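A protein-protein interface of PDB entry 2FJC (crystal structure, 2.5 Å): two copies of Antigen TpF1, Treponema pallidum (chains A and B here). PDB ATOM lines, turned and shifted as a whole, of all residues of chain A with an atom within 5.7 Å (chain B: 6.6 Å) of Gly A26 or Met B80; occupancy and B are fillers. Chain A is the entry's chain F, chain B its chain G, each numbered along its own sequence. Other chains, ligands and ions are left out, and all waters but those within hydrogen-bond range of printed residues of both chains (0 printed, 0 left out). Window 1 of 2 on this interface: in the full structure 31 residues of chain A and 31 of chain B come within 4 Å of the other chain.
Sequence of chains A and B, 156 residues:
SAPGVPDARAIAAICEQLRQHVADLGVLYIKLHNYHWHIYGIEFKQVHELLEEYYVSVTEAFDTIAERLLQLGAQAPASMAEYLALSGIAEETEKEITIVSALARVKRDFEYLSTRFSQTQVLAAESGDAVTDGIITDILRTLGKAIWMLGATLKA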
ATOM      1  N   HIS A  21     -21.182  11.804  -7.728  1.00  0.00           N
ATOM      2  CA  HIS A  21     -19.768  11.536  -7.527  1.00  0.00           C
ATOM      3  C   HIS A  21     -19.525  11.015  -6.111  1.00  0.00           C
ATOM      4  O   HIS A  21     -18.776  10.066  -5.912  1.00  0.00           O
ATOM      5  CB  HIS A  21     -18.932  12.795  -7.736  1.00  0.00           C
ATOM      6  CG  HIS A  21     -19.012  13.356  -9.118  1.00  0.00           C
ATOM      7  ND1 HIS A  21     -19.156  12.563 -10.232  1.00  0.00           N
ATOM      8  CD2 HIS A  21     -18.918  14.629  -9.570  1.00  0.00           C
ATOM      9  CE1 HIS A  21     -19.147  13.322 -11.314  1.00  0.00           C
ATOM     10  NE2 HIS A  21     -19.003  14.579 -10.939  1.00  0.00           N
ATOM     11  N   VAL A  22     -20.159  11.642  -5.130  1.00  0.00           N
ATOM     12  CA  VAL A  22     -19.991  11.210  -3.754  1.00  0.00           C
ATOM     13  C   VAL A  22     -20.442   9.759  -3.625  1.00  0.00           C
ATOM     14  O   VAL A  22     -19.758   8.934  -3.014  1.00  0.00           O
ATOM     15  CB  VAL A  22     -20.796  12.107  -2.790  1.00  0.00           C
ATOM     16  CG1 VAL A  22     -20.745  11.546  -1.384  1.00  0.00           C
ATOM     17  CG2 VAL A  22     -20.228  13.520  -2.815  1.00  0.00           C
ATOM     18  N   ALA A  23     -21.586   9.442  -4.224  1.00  0.00           N
ATOM     19  CA  ALA A  23     -22.117   8.087  -4.162  1.00  0.00           C
ATOM     20  C   ALA A  23     -21.164   7.100  -4.822  1.00  0.00           C
ATOM     21  O   ALA A  23     -20.875   6.034  -4.269  1.00  0.00           O
ATOM     22  CB  ALA A  23     -23.484   8.025  -4.841  1.00  0.00           C
ATOM     23  N   ASP A  24     -20.670   7.448  -6.007  1.00  0.00           N
ATOM     24  CA  ASP A  24     -19.761   6.557  -6.710  1.00  0.00           C
ATOM     25  C   ASP A  24     -18.451   6.380  -5.952  1.00  0.00           C
ATOM     26  O   ASP A  24     -17.940   5.269  -5.848  1.00  0.00           O
ATOM     27  CB  ASP A  24     -19.483   7.067  -8.132  1.00  0.00           C
ATOM     28  CG  ASP A  24     -20.683   6.917  -9.049  1.00  0.00           C
ATOM     29  OD1 ASP A  24     -21.546   6.055  -8.771  1.00  0.00           O
ATOM     30  OD2 ASP A  24     -20.760   7.645 -10.059  1.00  0.00           O
ATOM     31  N   LEU A  25     -17.918   7.475  -5.422  1.00  0.00           N
ATOM     32  CA  LEU A  25     -16.678   7.428  -4.671  1.00  0.00           C
ATOM     33  C   LEU A  25     -16.885   6.541  -3.444  1.00  0.00           C
ATOM     34  O   LEU A  25     -16.052   5.692  -3.137  1.00  0.00           O
ATOM     35  CB  LEU A  25     -16.265   8.844  -4.258  1.00  0.00           C
ATOM     36  CG  LEU A  25     -15.171   9.588  -5.034  1.00  0.00           C
ATOM     37  CD1 LEU A  25     -14.813   8.884  -6.310  1.00  0.00           C
ATOM     38  CD2 LEU A  25     -15.635  10.990  -5.309  1.00  0.00           C
ATOM     39  N   GLY A  26     -18.006   6.740  -2.752  1.00  0.00           N
ATOM     40  CA  GLY A  26     -18.299   5.934  -1.578  1.00  0.00           C
ATOM     41  C   GLY A  26     -18.303   4.441  -1.903  1.00  0.00           C
ATOM     42  O   GLY A  26     -17.710   3.635  -1.190  1.00  0.00           O
ATOM     43  N   VAL A  27     -18.970   4.071  -2.991  1.00  0.00           N
ATOM     44  CA  VAL A  27     -19.039   2.683  -3.405  1.00  0.00           C
ATOM     45  C   VAL A  27     -17.659   2.179  -3.809  1.00  0.00           C
ATOM     46  O   VAL A  27     -17.276   1.059  -3.481  1.00  0.00           O
ATOM     47  CB  VAL A  27     -20.015   2.512  -4.589  1.00  0.00           C
ATOM     48  CG1 VAL A  27     -19.885   1.138  -5.196  1.00  0.00           C
ATOM     49  CG2 VAL A  27     -21.438   2.741  -4.118  1.00  0.00           C
ATOM     50  N   LEU A  28     -16.904   3.011  -4.511  1.00  0.00           N
ATOM     51  CA  LEU A  28     -15.572   2.618  -4.947  1.00  0.00           C
ATOM     52  C   LEU A  28     -14.670   2.377  -3.741  1.00  0.00           C
ATOM     53  O   LEU A  28     -13.870   1.434  -3.720  1.00  0.00           O
ATOM     54  CB  LEU A  28     -14.956   3.712  -5.829  1.00  0.00           C
ATOM     55  CG  LEU A  28     -14.255   3.259  -7.109  1.00  0.00           C
ATOM     56  CD1 LEU A  28     -13.268   4.331  -7.503  1.00  0.00           C
ATOM     57  CD2 LEU A  28     -13.539   1.944  -6.904  1.00  0.00           C
ATOM     58  N   TYR A  29     -14.803   3.244  -2.741  1.00  0.00           N
ATOM     59  CA  TYR A  29     -14.012   3.149  -1.526  1.00  0.00           C
ATOM     60  C   TYR A  29     -14.072   1.746  -0.932  1.00  0.00           C
ATOM     61  O   TYR A  29     -13.044   1.160  -0.599  1.00  0.00           O
ATOM     62  CB  TYR A  29     -14.513   4.153  -0.495  1.00  0.00           C
ATOM     63  CG  TYR A  29     -13.724   4.149   0.794  1.00  0.00           C
ATOM     64  CD1 TYR A  29     -12.413   4.619   0.834  1.00  0.00           C
ATOM     65  CD2 TYR A  29     -14.293   3.677   1.981  1.00  0.00           C
ATOM     66  CE1 TYR A  29     -11.686   4.623   2.028  1.00  0.00           C
ATOM     67  CE2 TYR A  29     -13.577   3.679   3.178  1.00  0.00           C
ATOM     68  CZ  TYR A  29     -12.274   4.155   3.194  1.00  0.00           C
ATOM     69  OH  TYR A  29     -11.567   4.190   4.374  1.00  0.00           O
ATOM     70  N   ILE A  30     -15.278   1.203  -0.802  1.00  0.00           N
ATOM     71  CA  ILE A  30     -15.425  -0.126  -0.234  1.00  0.00           C
ATOM     72  C   ILE A  30     -15.039  -1.208  -1.228  1.00  0.00           C
ATOM     73  O   ILE A  30     -14.490  -2.232  -0.850  1.00  0.00           O
ATOM     74  CB  ILE A  30     -16.860  -0.331   0.291  1.00  0.00           C
ATOM     75  CG1 ILE A  30     -17.028   0.452   1.604  1.00  0.00           C
ATOM     76  CG2 ILE A  30     -17.154  -1.817   0.477  1.00  0.00           C
ATOM     77  CD1 ILE A  30     -18.462   0.555   2.070  1.00  0.00           C
ATOM     78  N   LYS A  31     -15.302  -0.963  -2.504  1.00  0.00           N
ATOM     79  CA  LYS A  31     -14.947  -1.908  -3.544  1.00  0.00           C
ATOM     80  C   LYS A  31     -13.429  -2.092  -3.548  1.00  0.00           C
ATOM     81  O   LYS A  31     -12.938  -3.208  -3.699  1.00  0.00           O
ATOM     82  CB  LYS A  31     -15.424  -1.384  -4.899  1.00  0.00           C
ATOM     83  CG  LYS A  31     -15.433  -2.411  -6.012  1.00  0.00           C
ATOM     84  CD  LYS A  31     -16.185  -1.858  -7.210  1.00  0.00           C
ATOM     85  CE  LYS A  31     -16.204  -2.848  -8.365  1.00  0.00           C
ATOM     86  NZ  LYS A  31     -16.920  -2.295  -9.552  1.00  0.00           N
ATOM     87  N   VAL A  58      -9.291   7.995  -2.978  1.00  0.00           N
ATOM     88  CA  VAL A  58     -10.703   8.049  -3.289  1.00  0.00           C
ATOM     89  C   VAL A  58     -11.493   8.716  -2.174  1.00  0.00           C
ATOM     90  O   VAL A  58     -12.374   9.540  -2.440  1.00  0.00           O
ATOM     91  CB  VAL A  58     -11.270   6.620  -3.548  1.00  0.00           C
ATOM     92  CG1 VAL A  58     -12.794   6.593  -3.350  1.00  0.00           C
ATOM     93  CG2 VAL A  58     -10.913   6.180  -4.963  1.00  0.00           C
ATOM     94  N   PHE A  62     -13.757  11.938  -2.163  1.00  0.00           N
ATOM     95  CA  PHE A  62     -15.072  11.739  -1.573  1.00  0.00           C
ATOM     96  C   PHE A  62     -15.399  12.928  -0.679  1.00  0.00           C
ATOM     97  O   PHE A  62     -16.444  13.568  -0.824  1.00  0.00           O
ATOM     98  CB  PHE A  62     -15.044  10.460  -0.724  1.00  0.00           C
ATOM     99  CG  PHE A  62     -16.306  10.189   0.056  1.00  0.00           C
ATOM    100  CD1 PHE A  62     -17.445   9.697  -0.575  1.00  0.00           C
ATOM    101  CD2 PHE A  62     -16.314  10.313   1.444  1.00  0.00           C
ATOM    102  CE1 PHE A  62     -18.570   9.316   0.165  1.00  0.00           C
ATOM    103  CE2 PHE A  62     -17.434   9.936   2.199  1.00  0.00           C
ATOM    104  CZ  PHE A  62     -18.562   9.434   1.558  1.00  0.00           C
ATOM    105  N   MET A  80     -25.231   4.580   3.094  1.00  0.00           N
ATOM    106  CA  MET A  80     -25.011   3.564   2.082  1.00  0.00           C
ATOM    107  C   MET A  80     -26.285   3.356   1.262  1.00  0.00           C
ATOM    108  O   MET A  80     -26.231   3.078   0.054  1.00  0.00           O
ATOM    109  CB  MET A  80     -24.582   2.266   2.746  1.00  0.00           C
ATOM    110  CG  MET A  80     -23.284   2.411   3.511  1.00  0.00           C
ATOM    111  SD  MET A  80     -22.751   0.876   4.197  1.00  0.00           S
ATOM    112  CE  MET A  80     -21.120   1.245   4.697  1.00  0.00           C
ATOM    113  N   TYR A  83     -26.221   5.946  -1.361  1.00  0.00           N
ATOM    114  CA  TYR A  83     -25.148   5.679  -2.306  1.00  0.00           C
ATOM    115  C   TYR A  83     -25.526   4.562  -3.258  1.00  0.00           C
ATOM    116  O   TYR A  83     -25.321   4.668  -4.470  1.00  0.00           O
ATOM    117  CB  TYR A  83     -23.850   5.327  -1.577  1.00  0.00           C
ATOM    118  CG  TYR A  83     -23.309   6.440  -0.710  1.00  0.00           C
ATOM    119  CD1 TYR A  83     -23.607   7.773  -0.987  1.00  0.00           C
ATOM    120  CD2 TYR A  83     -22.488   6.162   0.380  1.00  0.00           C
ATOM    121  CE1 TYR A  83     -23.105   8.796  -0.195  1.00  0.00           C
ATOM    122  CE2 TYR A  83     -21.981   7.181   1.179  1.00  0.00           C
ATOM    123  CZ  TYR A  83     -22.296   8.492   0.886  1.00  0.00           C
ATOM    124  OH  TYR A  83     -21.815   9.494   1.691  1.00  0.00           O
ATOM    125  N   LEU A  84     -26.086   3.486  -2.721  1.00  0.00           N
ATOM    126  CA  LEU A  84     -26.482   2.378  -3.570  1.00  0.00           C
ATOM    127  C   LEU A  84     -27.575   2.809  -4.547  1.00  0.00           C
ATOM    128  O   LEU A  84     -27.687   2.270  -5.654  1.00  0.00           O
ATOM    129  CB  LEU A  84     -26.962   1.209  -2.713  1.00  0.00           C
ATOM    130  CG  LEU A  84     -25.877   0.460  -1.946  1.00  0.00           C
ATOM    131  CD1 LEU A  84     -26.508  -0.682  -1.159  1.00  0.00           C
ATOM    132  CD2 LEU A  84     -24.842  -0.070  -2.921  1.00  0.00           C
ATOM    133  N   GLU A  91     -21.115  -2.985  -7.135  1.00  0.00           N
ATOM    134  CA  GLU A  91     -20.315  -3.474  -6.032  1.00  0.00           C
ATOM    135  C   GLU A  91     -19.688  -4.809  -6.404  1.00  0.00           C
ATOM    136  O   GLU A  91     -20.229  -5.542  -7.229  1.00  0.00           O
ATOM    137  CB  GLU A  91     -21.193  -3.625  -4.799  1.00  0.00           C
ATOM    138  CG  GLU A  91     -21.723  -2.299  -4.278  1.00  0.00           C
ATOM    139  CD  GLU A  91     -22.032  -2.344  -2.801  1.00  0.00           C
ATOM    140  OE1 GLU A  91     -22.971  -3.071  -2.414  1.00  0.00           O
ATOM    141  OE2 GLU A  91     -21.331  -1.659  -2.024  1.00  0.00           O
ATOM    142  N   VAL B  27     -20.633   1.005   8.317  1.00  0.00           N
ATOM    143  CA  VAL B  27     -21.811   1.863   8.399  1.00  0.00           C
ATOM    144  C   VAL B  27     -21.518   3.103   9.236  1.00  0.00           C
ATOM    145  O   VAL B  27     -21.949   4.204   8.900  1.00  0.00           O
ATOM    146  CB  VAL B  27     -23.016   1.086   9.016  1.00  0.00           C
ATOM    147  CG1 VAL B  27     -24.144   2.031   9.351  1.00  0.00           C
ATOM    148  CG2 VAL B  27     -23.505   0.030   8.030  1.00  0.00           C
ATOM    149  N   ILE B  30     -19.481   5.968   7.385  1.00  0.00           N
ATOM    150  CA  ILE B  30     -20.253   6.902   6.580  1.00  0.00           C
ATOM    151  C   ILE B  30     -21.174   7.763   7.431  1.00  0.00           C
ATOM    152  O   ILE B  30     -21.386   8.937   7.140  1.00  0.00           O
ATOM    153  CB  ILE B  30     -21.036   6.133   5.500  1.00  0.00           C
ATOM    154  CG1 ILE B  30     -20.034   5.647   4.446  1.00  0.00           C
ATOM    155  CG2 ILE B  30     -22.145   7.000   4.906  1.00  0.00           C
ATOM    156  CD1 ILE B  30     -20.627   4.728   3.420  1.00  0.00           C
ATOM    157  N   ALA B  78     -17.451  -7.262   1.915  1.00  0.00           N
ATOM    158  CA  ALA B  78     -16.882  -6.119   1.223  1.00  0.00           C
ATOM    159  C   ALA B  78     -17.802  -5.431   0.229  1.00  0.00           C
ATOM    160  O   ALA B  78     -17.478  -5.308  -0.946  1.00  0.00           O
ATOM    161  CB  ALA B  78     -15.596  -6.551   0.533  1.00  0.00           C
ATOM    162  N   SER B  79     -18.949  -4.977   0.709  1.00  0.00           N
ATOM    163  CA  SER B  79     -19.904  -4.280  -0.134  1.00  0.00           C
ATOM    164  C   SER B  79     -20.917  -3.633   0.784  1.00  0.00           C
ATOM    165  O   SER B  79     -21.199  -4.148   1.874  1.00  0.00           O
ATOM    166  CB  SER B  79     -20.621  -5.254  -1.071  1.00  0.00           C
ATOM    167  OG  SER B  79     -21.517  -6.085  -0.352  1.00  0.00           O
ATOM    168  N   MET B  80     -21.468  -2.507   0.355  1.00  0.00           N
ATOM    169  CA  MET B  80     -22.455  -1.832   1.167  1.00  0.00           C
ATOM    170  C   MET B  80     -23.696  -2.711   1.327  1.00  0.00           C
ATOM    171  O   MET B  80     -24.354  -2.696   2.374  1.00  0.00           O
ATOM    172  CB  MET B  80     -22.810  -0.495   0.531  1.00  0.00           C
ATOM    173  CG  MET B  80     -21.624   0.461   0.489  1.00  0.00           C
ATOM    174  SD  MET B  80     -22.068   2.015  -0.258  1.00  0.00           S
ATOM    175  CE  MET B  80     -20.594   2.978   0.064  1.00  0.00           C
ATOM    176  N   ALA B  81     -24.011  -3.486   0.293  1.00  0.00           N
ATOM    177  CA  ALA B  81     -25.171  -4.370   0.346  1.00  0.00           C
ATOM    178  C   ALA B  81     -25.035  -5.327   1.533  1.00  0.00           C
ATOM    179  O   ALA B  81     -25.958  -5.478   2.330  1.00  0.00           O
ATOM    180  CB  ALA B  81     -25.294  -5.153  -0.950  1.00  0.00           C
ATOM    181  N   GLU B  82     -23.876  -5.964   1.656  1.00  0.00           N
ATOM    182  CA  GLU B  82     -23.644  -6.884   2.763  1.00  0.00           C
ATOM    183  C   GLU B  82     -23.639  -6.146   4.094  1.00  0.00           C
ATOM    184  O   GLU B  82     -24.193  -6.632   5.076  1.00  0.00           O
ATOM    185  CB  GLU B  82     -22.308  -7.617   2.615  1.00  0.00           C
ATOM    186  CG  GLU B  82     -22.118  -8.357   1.314  1.00  0.00           C
ATOM    187  CD  GLU B  82     -20.714  -8.931   1.193  1.00  0.00           C
ATOM    188  OE1 GLU B  82     -20.450  -9.995   1.798  1.00  0.00           O
ATOM    189  OE2 GLU B  82     -19.868  -8.307   0.507  1.00  0.00           O
ATOM    190  N   TYR B  83     -23.005  -4.977   4.133  1.00  0.00           N
ATOM    191  CA  TYR B  83     -22.944  -4.210   5.376  1.00  0.00           C
ATOM    192  C   TYR B  83     -24.330  -3.844   5.878  1.00  0.00           C
ATOM    193  O   TYR B  83     -24.620  -3.993   7.066  1.00  0.00           O
ATOM    194  CB  TYR B  83     -22.104  -2.939   5.200  1.00  0.00           C
ATOM    195  CG  TYR B  83     -20.652  -3.210   4.881  1.00  0.00           C
ATOM    196  CD1 TYR B  83     -20.040  -4.394   5.292  1.00  0.00           C
ATOM    197  CD2 TYR B  83     -19.881  -2.276   4.181  1.00  0.00           C
ATOM    198  CE1 TYR B  83     -18.700  -4.643   5.012  1.00  0.00           C
ATOM    199  CE2 TYR B  83     -18.542  -2.516   3.901  1.00  0.00           C
ATOM    200  CZ  TYR B  83     -17.960  -3.700   4.320  1.00  0.00           C
ATOM    201  OH  TYR B  83     -16.638  -3.957   4.057  1.00  0.00           O
ATOM    202  N   LEU B  84     -25.185  -3.369   4.977  1.00  0.00           N
ATOM    203  CA  LEU B  84     -26.536  -3.003   5.361  1.00  0.00           C
ATOM    204  C   LEU B  84     -27.305  -4.232   5.847  1.00  0.00           C
ATOM    205  O   LEU B  84     -28.198  -4.126   6.694  1.00  0.00           O
ATOM    206  CB  LEU B  84     -27.264  -2.353   4.181  1.00  0.00           C
ATOM    207  CG  LEU B  84     -26.802  -0.933   3.839  1.00  0.00           C
ATOM    208  CD1 LEU B  84     -27.571  -0.426   2.630  1.00  0.00           C
ATOM    209  CD2 LEU B  84     -27.024  -0.017   5.039  1.00  0.00           C
ATOM    210  N   ALA B  85     -26.938  -5.400   5.333  1.00  0.00           N
ATOM    211  CA  ALA B  85     -27.599  -6.640   5.716  1.00  0.00           C
ATOM    212  C   ALA B  85     -27.102  -7.180   7.054  1.00  0.00           C
ATOM    213  O   ALA B  85     -27.852  -7.833   7.784  1.00  0.00           O
ATOM    214  CB  ALA B  85     -27.396  -7.694   4.622  1.00  0.00           C
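N of Ala B81 sits at hydrogen-bond distance from OE1 of Glu A91 (2.9 Å). OE2 of Glu A91 lies within hydrogen-bond range of N of Met B80 (2.5 Å).
The side-chain hydroxyl (OG) of Ser B79 sits close to the side-chain carboxylate (OE2) of Glu B82, 2.9 Å away. OE2 of Glu B82 sits at hydrogen-bond distance from N of Ala B78 (3.0 Å).
Among the printed residues, merely in contact across the chains: Gly A26 with Met B80, Glu A91 with Ser B79, Met A80 with Ile B30, Ile A30 with Met B80, Ile A30 with Tyr B83, Tyr A83 with Ile B30, Val A27 with Met B80, Ile A30 with Ser B79, Met A80 with Val B27, Ile A30 with Ala B78, Tyr A83 with Met B80, Met A80 with Tyr B83, Met A80 with Met B80 and Leu A84 with Leu B84.
Gly A26 touches just one residue of chain B: Met B80 (3.2 Å). Of chain A, only Gly A26 (3.2 Å), Val A27 (3.6 Å), Ile A30 (3.5 Å), Met A80 (3.9 Å), Tyr A83 (3.7 Å) and Glu A91 (2.5 Å) come within 4 Å of Met B80. Of the printed residues of chain B, Ile A30 touches Ala B78 (3.7 Å), Ser B79 (3.6 Å), Met B80 (3.5 Å) and Tyr B83 (3.6 Å). Of the printed residues of chain A, Ala B78 touches Ile A30 (3.7 Å). Phe A62 touches none of the printed residues of chain B. His A21 touches none of the printed residues of chain B.
Printed residues of chain B that touch a printed residue of chain A: Val B27, Ile B30, Ala B78, Ser B79, Met B80, Ala B81, Tyr B83 and Leu B84. Hydrophobic or aromatic side chains of chain B within 4 Å of the printed part of chain A: Val B27, Ile B30, Met B80, Ala B81, Tyr B83 and Leu B84. Among the printed residues, no Asp or Glu carboxylate lies within 4 Å of a Lys or Arg side-chain nitrogen of the other chain.
Val A27 touches Met B80, and with the chains exchanged Met A80 touches Val B27. Ile A30 touches Met B80, and with the chains exchanged Met A80 touches Ile B30. Ile A30 touches Tyr B83, and with the chains exchanged Tyr A83 touches Ile B30. Leu A84 touches its own counterpart, Leu B84. 5 positions are printed for both chains.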
